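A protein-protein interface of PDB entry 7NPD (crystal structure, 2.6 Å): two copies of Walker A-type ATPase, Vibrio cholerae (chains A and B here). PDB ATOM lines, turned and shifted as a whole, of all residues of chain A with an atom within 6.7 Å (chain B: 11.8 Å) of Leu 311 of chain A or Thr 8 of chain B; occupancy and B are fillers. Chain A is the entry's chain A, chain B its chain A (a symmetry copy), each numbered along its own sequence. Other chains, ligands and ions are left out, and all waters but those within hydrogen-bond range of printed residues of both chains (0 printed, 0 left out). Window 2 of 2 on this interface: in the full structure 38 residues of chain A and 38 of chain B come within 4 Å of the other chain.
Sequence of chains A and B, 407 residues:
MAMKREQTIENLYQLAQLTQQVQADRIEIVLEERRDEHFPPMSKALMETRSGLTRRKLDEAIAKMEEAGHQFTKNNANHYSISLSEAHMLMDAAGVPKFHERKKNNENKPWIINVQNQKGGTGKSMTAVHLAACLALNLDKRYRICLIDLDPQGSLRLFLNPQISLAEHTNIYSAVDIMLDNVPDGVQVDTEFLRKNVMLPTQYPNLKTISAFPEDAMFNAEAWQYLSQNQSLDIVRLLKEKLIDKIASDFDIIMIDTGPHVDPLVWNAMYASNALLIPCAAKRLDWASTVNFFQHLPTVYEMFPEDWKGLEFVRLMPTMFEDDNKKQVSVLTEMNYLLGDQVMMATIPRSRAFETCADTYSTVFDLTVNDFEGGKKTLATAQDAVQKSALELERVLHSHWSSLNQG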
ATOM      1  N   MET A 270      22.148  17.374  18.648  1.00  0.00           N
ATOM      2  CA  MET A 270      22.209  17.186  17.199  1.00  0.00           C
ATOM      3  C   MET A 270      22.952  15.906  16.837  1.00  0.00           C
ATOM      4  O   MET A 270      22.601  15.224  15.871  1.00  0.00           O
ATOM      5  CB  MET A 270      22.915  18.376  16.571  1.00  0.00           C
ATOM      6  CG  MET A 270      22.076  19.609  16.416  1.00  0.00           C
ATOM      7  SD  MET A 270      23.184  20.996  16.098  1.00  0.00           S
ATOM      8  CE  MET A 270      22.034  22.314  15.682  1.00  0.00           C
ATOM      9  N   SER A 273      20.909  12.874  17.246  1.00  0.00           N
ATOM     10  CA  SER A 273      19.660  13.187  16.574  1.00  0.00           C
ATOM     11  C   SER A 273      19.806  12.924  15.101  1.00  0.00           C
ATOM     12  O   SER A 273      20.731  13.443  14.453  1.00  0.00           O
ATOM     13  CB  SER A 273      19.440  14.668  16.738  1.00  0.00           C
ATOM     14  OG  SER A 273      18.486  15.199  15.782  1.00  0.00           O
ATOM     15  N   ASN A 274      18.814  12.282  14.573  1.00  0.00           N
ATOM     16  CA  ASN A 274      18.867  11.793  13.215  1.00  0.00           C
ATOM     17  C   ASN A 274      17.753  12.365  12.345  1.00  0.00           C
ATOM     18  O   ASN A 274      17.348  11.749  11.346  1.00  0.00           O
ATOM     19  CB  ASN A 274      18.856  10.273  13.226  1.00  0.00           C
ATOM     20  CG  ASN A 274      17.592   9.686  13.780  1.00  0.00           C
ATOM     21  OD1 ASN A 274      16.480  10.179  13.535  1.00  0.00           O
ATOM     22  ND2 ASN A 274      17.752   8.597  14.540  1.00  0.00           N
ATOM     23  N   ALA A 275      17.266  13.553  12.713  1.00  0.00           N
ATOM     24  CA  ALA A 275      16.493  14.394  11.813  1.00  0.00           C
ATOM     25  C   ALA A 275      16.256  15.707  12.514  1.00  0.00           C
ATOM     26  O   ALA A 275      16.330  15.786  13.742  1.00  0.00           O
ATOM     27  CB  ALA A 275      15.165  13.783  11.427  1.00  0.00           C
ATOM     28  N   LEU A 276      15.975  16.731  11.719  1.00  0.00           N
ATOM     29  CA  LEU A 276      15.907  18.089  12.209  1.00  0.00           C
ATOM     30  C   LEU A 276      14.582  18.670  11.825  1.00  0.00           C
ATOM     31  O   LEU A 276      14.070  18.382  10.741  1.00  0.00           O
ATOM     32  CB  LEU A 276      17.002  18.920  11.622  1.00  0.00           C
ATOM     33  CG  LEU A 276      17.741  19.683  12.696  1.00  0.00           C
ATOM     34  CD1 LEU A 276      18.097  18.705  13.784  1.00  0.00           C
ATOM     35  CD2 LEU A 276      19.030  20.285  12.125  1.00  0.00           C
ATOM     36  N   LEU A 277      14.049  19.511  12.690  1.00  0.00           N
ATOM     37  CA  LEU A 277      12.766  20.103  12.377  1.00  0.00           C
ATOM     38  C   LEU A 277      12.827  21.507  12.944  1.00  0.00           C
ATOM     39  O   LEU A 277      13.163  21.680  14.121  1.00  0.00           O
ATOM     40  CB  LEU A 277      11.623  19.251  12.959  1.00  0.00           C
ATOM     41  CG  LEU A 277      10.164  19.683  13.131  1.00  0.00           C
ATOM     42  CD1 LEU A 277       9.599  20.182  11.805  1.00  0.00           C
ATOM     43  CD2 LEU A 277       9.359  18.470  13.655  1.00  0.00           C
ATOM     44  N   PRO A 298      26.553  24.173   8.645  1.00  0.00           N
ATOM     45  CA  PRO A 298      27.264  22.899   8.376  1.00  0.00           C
ATOM     46  C   PRO A 298      28.459  22.452   9.230  1.00  0.00           C
ATOM     47  O   PRO A 298      28.518  21.278   9.648  1.00  0.00           O
ATOM     48  CB  PRO A 298      27.709  23.074   6.925  1.00  0.00           C
ATOM     49  CG  PRO A 298      26.901  24.178   6.458  1.00  0.00           C
ATOM     50  CD  PRO A 298      26.836  25.114   7.590  1.00  0.00           C
ATOM     51  N   TYR A 301      27.963  20.419  12.665  1.00  0.00           N
ATOM     52  CA  TYR A 301      27.853  19.000  12.567  1.00  0.00           C
ATOM     53  C   TYR A 301      29.166  18.414  12.186  1.00  0.00           C
ATOM     54  O   TYR A 301      29.580  17.446  12.815  1.00  0.00           O
ATOM     55  CB  TYR A 301      26.839  18.641  11.483  1.00  0.00           C
ATOM     56  CG  TYR A 301      25.452  18.612  12.008  1.00  0.00           C
ATOM     57  CD1 TYR A 301      25.151  17.792  13.063  1.00  0.00           C
ATOM     58  CD2 TYR A 301      24.449  19.379  11.463  1.00  0.00           C
ATOM     59  CE1 TYR A 301      23.925  17.720  13.579  1.00  0.00           C
ATOM     60  CE2 TYR A 301      23.178  19.299  11.968  1.00  0.00           C
ATOM     61  CZ  TYR A 301      22.935  18.471  13.043  1.00  0.00           C
ATOM     62  OH  TYR A 301      21.682  18.395  13.581  1.00  0.00           O
ATOM     63  N   TRP A 308      29.206  10.168  13.406  1.00  0.00           N
ATOM     64  CA  TRP A 308      27.892  10.761  13.298  1.00  0.00           C
ATOM     65  C   TRP A 308      27.176  10.292  12.038  1.00  0.00           C
ATOM     66  O   TRP A 308      27.678  10.459  10.922  1.00  0.00           O
ATOM     67  CB  TRP A 308      27.970  12.271  13.322  1.00  0.00           C
ATOM     68  CG  TRP A 308      26.635  12.704  13.355  1.00  0.00           C
ATOM     69  CD1 TRP A 308      25.608  12.159  14.084  1.00  0.00           C
ATOM     70  CD2 TRP A 308      26.065  13.658  12.503  1.00  0.00           C
ATOM     71  NE1 TRP A 308      24.441  12.792  13.783  1.00  0.00           N
ATOM     72  CE2 TRP A 308      24.700  13.719  12.811  1.00  0.00           C
ATOM     73  CE3 TRP A 308      26.583  14.510  11.533  1.00  0.00           C
ATOM     74  CZ2 TRP A 308      23.863  14.590  12.201  1.00  0.00           C
ATOM     75  CZ3 TRP A 308      25.744  15.364  10.920  1.00  0.00           C
ATOM     76  CH2 TRP A 308      24.387  15.394  11.242  1.00  0.00           C
ATOM     77  N   LYS A 309      25.979   9.731  12.249  1.00  0.00           N
ATOM     78  CA  LYS A 309      25.062   9.077  11.322  1.00  0.00           C
ATOM     79  C   LYS A 309      24.322  10.047  10.407  1.00  0.00           C
ATOM     80  O   LYS A 309      23.223   9.703   9.925  1.00  0.00           O
ATOM     81  CB  LYS A 309      24.066   8.239  12.121  1.00  0.00           C
ATOM     82  N   GLY A 310      24.854  11.265  10.194  1.00  0.00           N
ATOM     83  CA  GLY A 310      24.238  12.155   9.232  1.00  0.00           C
ATOM     84  C   GLY A 310      22.829  12.491   9.654  1.00  0.00           C
ATOM     85  O   GLY A 310      22.352  12.093  10.718  1.00  0.00           O
ATOM     86  N   LEU A 311      22.148  13.225   8.798  1.00  0.00           N
ATOM     87  CA  LEU A 311      20.738  13.426   9.052  1.00  0.00           C
ATOM     88  C   LEU A 311      19.952  12.626   8.042  1.00  0.00           C
ATOM     89  O   LEU A 311      20.436  12.297   6.968  1.00  0.00           O
ATOM     90  CB  LEU A 311      20.372  14.915   9.046  1.00  0.00           C
ATOM     91  CG  LEU A 311      20.033  15.350  10.478  1.00  0.00           C
ATOM     92  CD1 LEU A 311      21.256  15.369  11.277  1.00  0.00           C
ATOM     93  CD2 LEU A 311      19.514  16.749  10.506  1.00  0.00           C
ATOM     94  N   GLU A 312      18.682  12.396   8.323  1.00  0.00           N
ATOM     95  CA  GLU A 312      17.914  11.711   7.328  1.00  0.00           C
ATOM     96  C   GLU A 312      17.246  12.869   6.609  1.00  0.00           C
ATOM     97  O   GLU A 312      17.816  13.461   5.704  1.00  0.00           O
ATOM     98  CB  GLU A 312      16.928  10.741   7.940  1.00  0.00           C
ATOM     99  CG  GLU A 312      17.625   9.602   8.534  1.00  0.00           C
ATOM    100  CD  GLU A 312      18.071   8.678   7.443  1.00  0.00           C
ATOM    101  OE1 GLU A 312      17.521   8.835   6.323  1.00  0.00           O
ATOM    102  OE2 GLU A 312      18.990   7.852   7.679  1.00  0.00           O
ATOM    103  N   PHE A 313      16.234  13.411   7.198  1.00  0.00           N
ATOM    104  CA  PHE A 313      15.633  14.565   6.592  1.00  0.00           C
ATOM    105  C   PHE A 313      15.874  15.744   7.509  1.00  0.00           C
ATOM    106  O   PHE A 313      16.508  15.629   8.564  1.00  0.00           O
ATOM    107  CB  PHE A 313      14.164  14.308   6.296  1.00  0.00           C
ATOM    108  CG  PHE A 313      13.318  14.123   7.514  1.00  0.00           C
ATOM    109  CD1 PHE A 313      12.235  14.944   7.737  1.00  0.00           C
ATOM    110  CD2 PHE A 313      13.585  13.105   8.416  1.00  0.00           C
ATOM    111  CE1 PHE A 313      11.452  14.758   8.853  1.00  0.00           C
ATOM    112  CE2 PHE A 313      12.791  12.906   9.533  1.00  0.00           C
ATOM    113  CZ  PHE A 313      11.741  13.750   9.752  1.00  0.00           C
ATOM    114  N   VAL A 314      15.372  16.892   7.076  1.00  0.00           N
ATOM    115  CA  VAL A 314      15.455  18.159   7.781  1.00  0.00           C
ATOM    116  C   VAL A 314      14.328  18.970   7.193  1.00  0.00           C
ATOM    117  O   VAL A 314      14.339  19.221   5.989  1.00  0.00           O
ATOM    118  CB  VAL A 314      16.780  18.888   7.491  1.00  0.00           C
ATOM    119  CG1 VAL A 314      16.584  20.429   7.655  1.00  0.00           C
ATOM    120  CG2 VAL A 314      17.876  18.381   8.335  1.00  0.00           C
ATOM    121  N   LYS B   4      25.423   8.055   6.246  1.00  0.00           N
ATOM    122  CA  LYS B   4      25.464   9.130   5.267  1.00  0.00           C
ATOM    123  C   LYS B   4      26.098  10.398   5.819  1.00  0.00           C
ATOM    124  O   LYS B   4      25.730  11.475   5.370  1.00  0.00           O
ATOM    125  CB  LYS B   4      24.049   9.458   4.769  1.00  0.00           C
ATOM    126  N   ARG B   5      27.029  10.265   6.780  1.00  0.00           N
ATOM    127  CA  ARG B   5      27.643  11.428   7.426  1.00  0.00           C
ATOM    128  C   ARG B   5      28.049  12.472   6.388  1.00  0.00           C
ATOM    129  O   ARG B   5      27.653  13.645   6.465  1.00  0.00           O
ATOM    130  CB  ARG B   5      28.850  10.981   8.274  1.00  0.00           C
ATOM    131  CG  ARG B   5      29.863  12.169   8.635  1.00  0.00           C
ATOM    132  CD  ARG B   5      31.270  11.596   9.126  1.00  0.00           C
ATOM    133  NE  ARG B   5      32.507  12.427   8.858  1.00  0.00           N
ATOM    134  CZ  ARG B   5      33.711  11.899   8.474  1.00  0.00           C
ATOM    135  NH1 ARG B   5      34.804  12.688   8.243  1.00  0.00           N
ATOM    136  NH2 ARG B   5      33.830  10.543   8.340  1.00  0.00           N
ATOM    137  N   GLU B   6      28.785  12.036   5.362  1.00  0.00           N
ATOM    138  CA  GLU B   6      29.265  12.960   4.339  1.00  0.00           C
ATOM    139  C   GLU B   6      28.107  13.636   3.600  1.00  0.00           C
ATOM    140  O   GLU B   6      28.038  14.870   3.525  1.00  0.00           O
ATOM    141  CB  GLU B   6      30.173  12.209   3.360  1.00  0.00           C
ATOM    142  N   GLN B   7      27.188  12.838   3.047  1.00  0.00           N
ATOM    143  CA  GLN B   7      26.169  13.363   2.139  1.00  0.00           C
ATOM    144  C   GLN B   7      25.340  14.469   2.786  1.00  0.00           C
ATOM    145  O   GLN B   7      24.944  15.438   2.119  1.00  0.00           O
ATOM    146  CB  GLN B   7      25.279  12.202   1.665  1.00  0.00           C
ATOM    147  N   THR B   8      25.070  14.344   4.079  1.00  0.00           N
ATOM    148  CA  THR B   8      24.221  15.314   4.752  1.00  0.00           C
ATOM    149  C   THR B   8      24.948  16.624   5.015  1.00  0.00           C
ATOM    150  O   THR B   8      24.361  17.692   4.831  1.00  0.00           O
ATOM    151  CB  THR B   8      23.683  14.707   6.033  1.00  0.00           C
ATOM    152  OG1 THR B   8      24.697  13.871   6.620  1.00  0.00           O
ATOM    153  CG2 THR B   8      22.416  13.952   5.727  1.00  0.00           C
ATOM    154  N   ILE B   9      26.224  16.567   5.411  1.00  0.00           N
ATOM    155  CA  ILE B   9      27.045  17.773   5.454  1.00  0.00           C
ATOM    156  C   ILE B   9      26.992  18.467   4.109  1.00  0.00           C
ATOM    157  O   ILE B   9      26.953  19.700   4.017  1.00  0.00           O
ATOM    158  CB  ILE B   9      28.506  17.413   5.779  1.00  0.00           C
ATOM    159  CG1 ILE B   9      28.726  16.849   7.184  1.00  0.00           C
ATOM    160  CG2 ILE B   9      29.338  18.642   5.787  1.00  0.00           C
ATOM    161  CD1 ILE B   9      30.224  16.200   7.346  1.00  0.00           C
ATOM    162  N   GLU B  10      27.090  17.679   3.043  1.00  0.00           N
ATOM    163  CA  GLU B  10      27.145  18.262   1.715  1.00  0.00           C
ATOM    164  C   GLU B  10      25.848  18.996   1.409  1.00  0.00           C
ATOM    165  O   GLU B  10      25.875  20.148   0.967  1.00  0.00           O
ATOM    166  CB  GLU B  10      27.444  17.164   0.700  1.00  0.00           C
ATOM    167  CG  GLU B  10      28.278  17.599  -0.590  1.00  0.00           C
ATOM    168  CD  GLU B  10      27.772  16.798  -1.820  1.00  0.00           C
ATOM    169  OE1 GLU B  10      27.853  17.371  -2.959  1.00  0.00           O
ATOM    170  OE2 GLU B  10      27.152  15.683  -1.588  1.00  0.00           O
ATOM    171  N   ASN B  11      24.699  18.382   1.720  1.00  0.00           N
ATOM    172  CA  ASN B  11      23.459  19.152   1.617  1.00  0.00           C
ATOM    173  C   ASN B  11      23.468  20.351   2.568  1.00  0.00           C
ATOM    174  O   ASN B  11      22.857  21.386   2.266  1.00  0.00           O
ATOM    175  CB  ASN B  11      22.241  18.247   1.883  1.00  0.00           C
ATOM    176  CG  ASN B  11      20.943  19.033   2.015  1.00  0.00           C
ATOM    177  OD1 ASN B  11      20.775  20.069   1.379  1.00  0.00           O
ATOM    178  ND2 ASN B  11      20.025  18.548   2.841  1.00  0.00           N
ATOM    179  N   LEU B  12      24.202  20.258   3.678  1.00  0.00           N
ATOM    180  CA  LEU B  12      24.180  21.325   4.669  1.00  0.00           C
ATOM    181  C   LEU B  12      24.888  22.571   4.150  1.00  0.00           C
ATOM    182  O   LEU B  12      24.310  23.654   4.163  1.00  0.00           O
ATOM    183  CB  LEU B  12      24.794  20.837   5.978  1.00  0.00           C
ATOM    184  N   TYR B  13      26.149  22.436   3.705  1.00  0.00           N
ATOM    185  CA  TYR B  13      26.826  23.542   3.023  1.00  0.00           C
ATOM    186  C   TYR B  13      26.033  23.969   1.812  1.00  0.00           C
ATOM    187  O   TYR B  13      26.011  25.146   1.449  1.00  0.00           O
ATOM    188  CB  TYR B  13      28.219  23.147   2.556  1.00  0.00           C
ATOM    189  CG  TYR B  13      29.235  22.942   3.615  1.00  0.00           C
ATOM    190  CD1 TYR B  13      29.857  23.994   4.268  1.00  0.00           C
ATOM    191  CD2 TYR B  13      29.545  21.669   3.991  1.00  0.00           C
ATOM    192  CE1 TYR B  13      30.807  23.747   5.259  1.00  0.00           C
ATOM    193  CE2 TYR B  13      30.461  21.421   4.943  1.00  0.00           C
ATOM    194  CZ  TYR B  13      31.093  22.439   5.590  1.00  0.00           C
ATOM    195  OH  TYR B  13      32.005  22.078   6.555  1.00  0.00           O
ATOM    196  N   GLN B  14      25.398  23.012   1.153  1.00  0.00           N
ATOM    197  CA  GLN B  14      24.584  23.362   0.013  1.00  0.00           C
ATOM    198  C   GLN B  14      23.535  24.359   0.423  1.00  0.00           C
ATOM    199  O   GLN B  14      23.274  25.326  -0.288  1.00  0.00           O
ATOM    200  CB  GLN B  14      23.944  22.120  -0.573  1.00  0.00           C
ATOM    201  N   LEU B  15      22.894  24.135   1.563  1.00  0.00           N
ATOM    202  CA  LEU B  15      21.965  25.157   2.057  1.00  0.00           C
ATOM    203  C   LEU B  15      22.695  26.310   2.747  1.00  0.00           C
ATOM    204  O   LEU B  15      22.165  27.406   2.854  1.00  0.00           O
ATOM    205  CB  LEU B  15      20.881  24.546   2.956  1.00  0.00           C
ATOM    206  CG  LEU B  15      19.640  24.792   2.070  1.00  0.00           C
ATOM    207  CD1 LEU B  15      18.184  24.520   2.651  1.00  0.00           C
ATOM    208  CD2 LEU B  15      19.617  26.245   1.621  1.00  0.00           C
ATOM    209  N   ALA B  16      23.882  26.074   3.258  1.00  0.00           N
ATOM    210  CA  ALA B  16      24.673  27.137   3.863  1.00  0.00           C
ATOM    211  C   ALA B  16      24.976  28.245   2.865  1.00  0.00           C
ATOM    212  O   ALA B  16      24.877  29.430   3.202  1.00  0.00           O
ATOM    213  CB  ALA B  16      25.970  26.543   4.414  1.00  0.00           C
ATOM    214  N   GLN B  17      25.367  27.869   1.644  1.00  0.00           N
ATOM    215  CA  GLN B  17      25.752  28.782   0.581  1.00  0.00           C
ATOM    216  C   GLN B  17      24.602  29.071  -0.371  1.00  0.00           C
ATOM    217  O   GLN B  17      24.558  30.138  -0.978  1.00  0.00           O
ATOM    218  CB  GLN B  17      26.924  28.192  -0.190  1.00  0.00           C
ATOM    219  N   LEU B  18      23.671  28.144  -0.538  1.00  0.00           N
ATOM    220  CA  LEU B  18      22.451  28.481  -1.258  1.00  0.00           C
ATOM    221  C   LEU B  18      21.733  29.636  -0.569  1.00  0.00           C
ATOM    222  O   LEU B  18      21.477  30.683  -1.175  1.00  0.00           O
ATOM    223  CB  LEU B  18      21.542  27.248  -1.356  1.00  0.00           C
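Hydrophobic or aromatic side chains of chain B that line the printed part of chain A: Leu 12, Tyr 13 and Ala 16. Of the 15 printed residues of chain A, 4 touch a printed residue of chain B. Hydrophobic or aromatic side chains of chain A within 4 Å of the printed part of chain B: Pro 298. Among the printed residues, 7 pairs touch across the chains. Among the printed residues, no Asp or Glu carboxylate lies within 4 Å of a Lys or Arg side-chain nitrogen of the other chain.
The side-chain hydroxyl (OG1) of Thr 8 of chain B sits close to the backbone NH (N) of Leu 311 of chain A, at 3.4 Å.
No position is printed for both chains. Of the 7 pairs that touch across the chains among the printed residues, none has its exchanged pair printed and touching as well.
Among the printed residues, merely in contact across the chains: Pro 298 of chain A with Leu 12 of chain B (3.5 Å), Pro 298 of chain A with Tyr 13 of chain B (3.3 Å), Pro 298 of chain A with Ala 16 of chain B (3.3 Å), Trp 308 of chain A with Arg 5 of chain B (2.9 Å), Gly 310 of chain A with Arg 5 of chain B (3.9 Å) and Gly 310 of chain A with Thr 8 of chain B (3.2 Å).
The backbone carbonyl oxygen of Lys 4 of chain B lies within hydrogen-bond range of the side-chain hydroxyl of Thr 8 of chain B, at 2.9 Å. The backbone carbonyl oxygen (O) of Arg 5 of chain B lies within hydrogen-bond range of the side-chain hydroxyl (OG1) of Thr 8 of chain B.
Leu 311 of chain A touches just one residue of chain B: Thr 8 (2.9 Å). Printed residues of chain A within 4 Å of Thr 8 of chain B: Gly 310 (3.2 Å) and Leu 311 (2.9 Å). No residue of chain B comes within 4 Å of Ala 275 of chain A. No residue of chain B comes within 4 Å of Leu 276 of chain A. Of chain B, only Arg 5 (3.9 Å) and Thr 8 (3.2 Å) come within 4 Å of Gly 310 of chain A. No residue of chain B comes within 4 Å of Glu 312 of chain A. Of the printed residues of chain B, Trp 308 of chain A touches Arg 5. Printed residues of chain A within 4 Å of Leu 12 of chain B: Pro 298. Of the printed residues of chain A, Ala 16 of chain B touches Pro 298. Printed residues of chain A within 4 Å of Tyr 13 of chain B: Pro 298. Of the printed residues of chain A, Arg 5 of chain B touches Trp 308 (2.9 Å) and Gly 310 (3.9 Å). Met 270 of chain A touches none of the printed residues of chain B. Asn 274 of chain A touches none of the printed residues of chain B. The nearest residue of chain A that does not touch Thr 8 of chain B is Glu 312 of chain A (4.6 Å). The nearest printed residue of chain B that does not touch Pro 298 of chain A is Ile 9 of chain B (4.5 Å).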
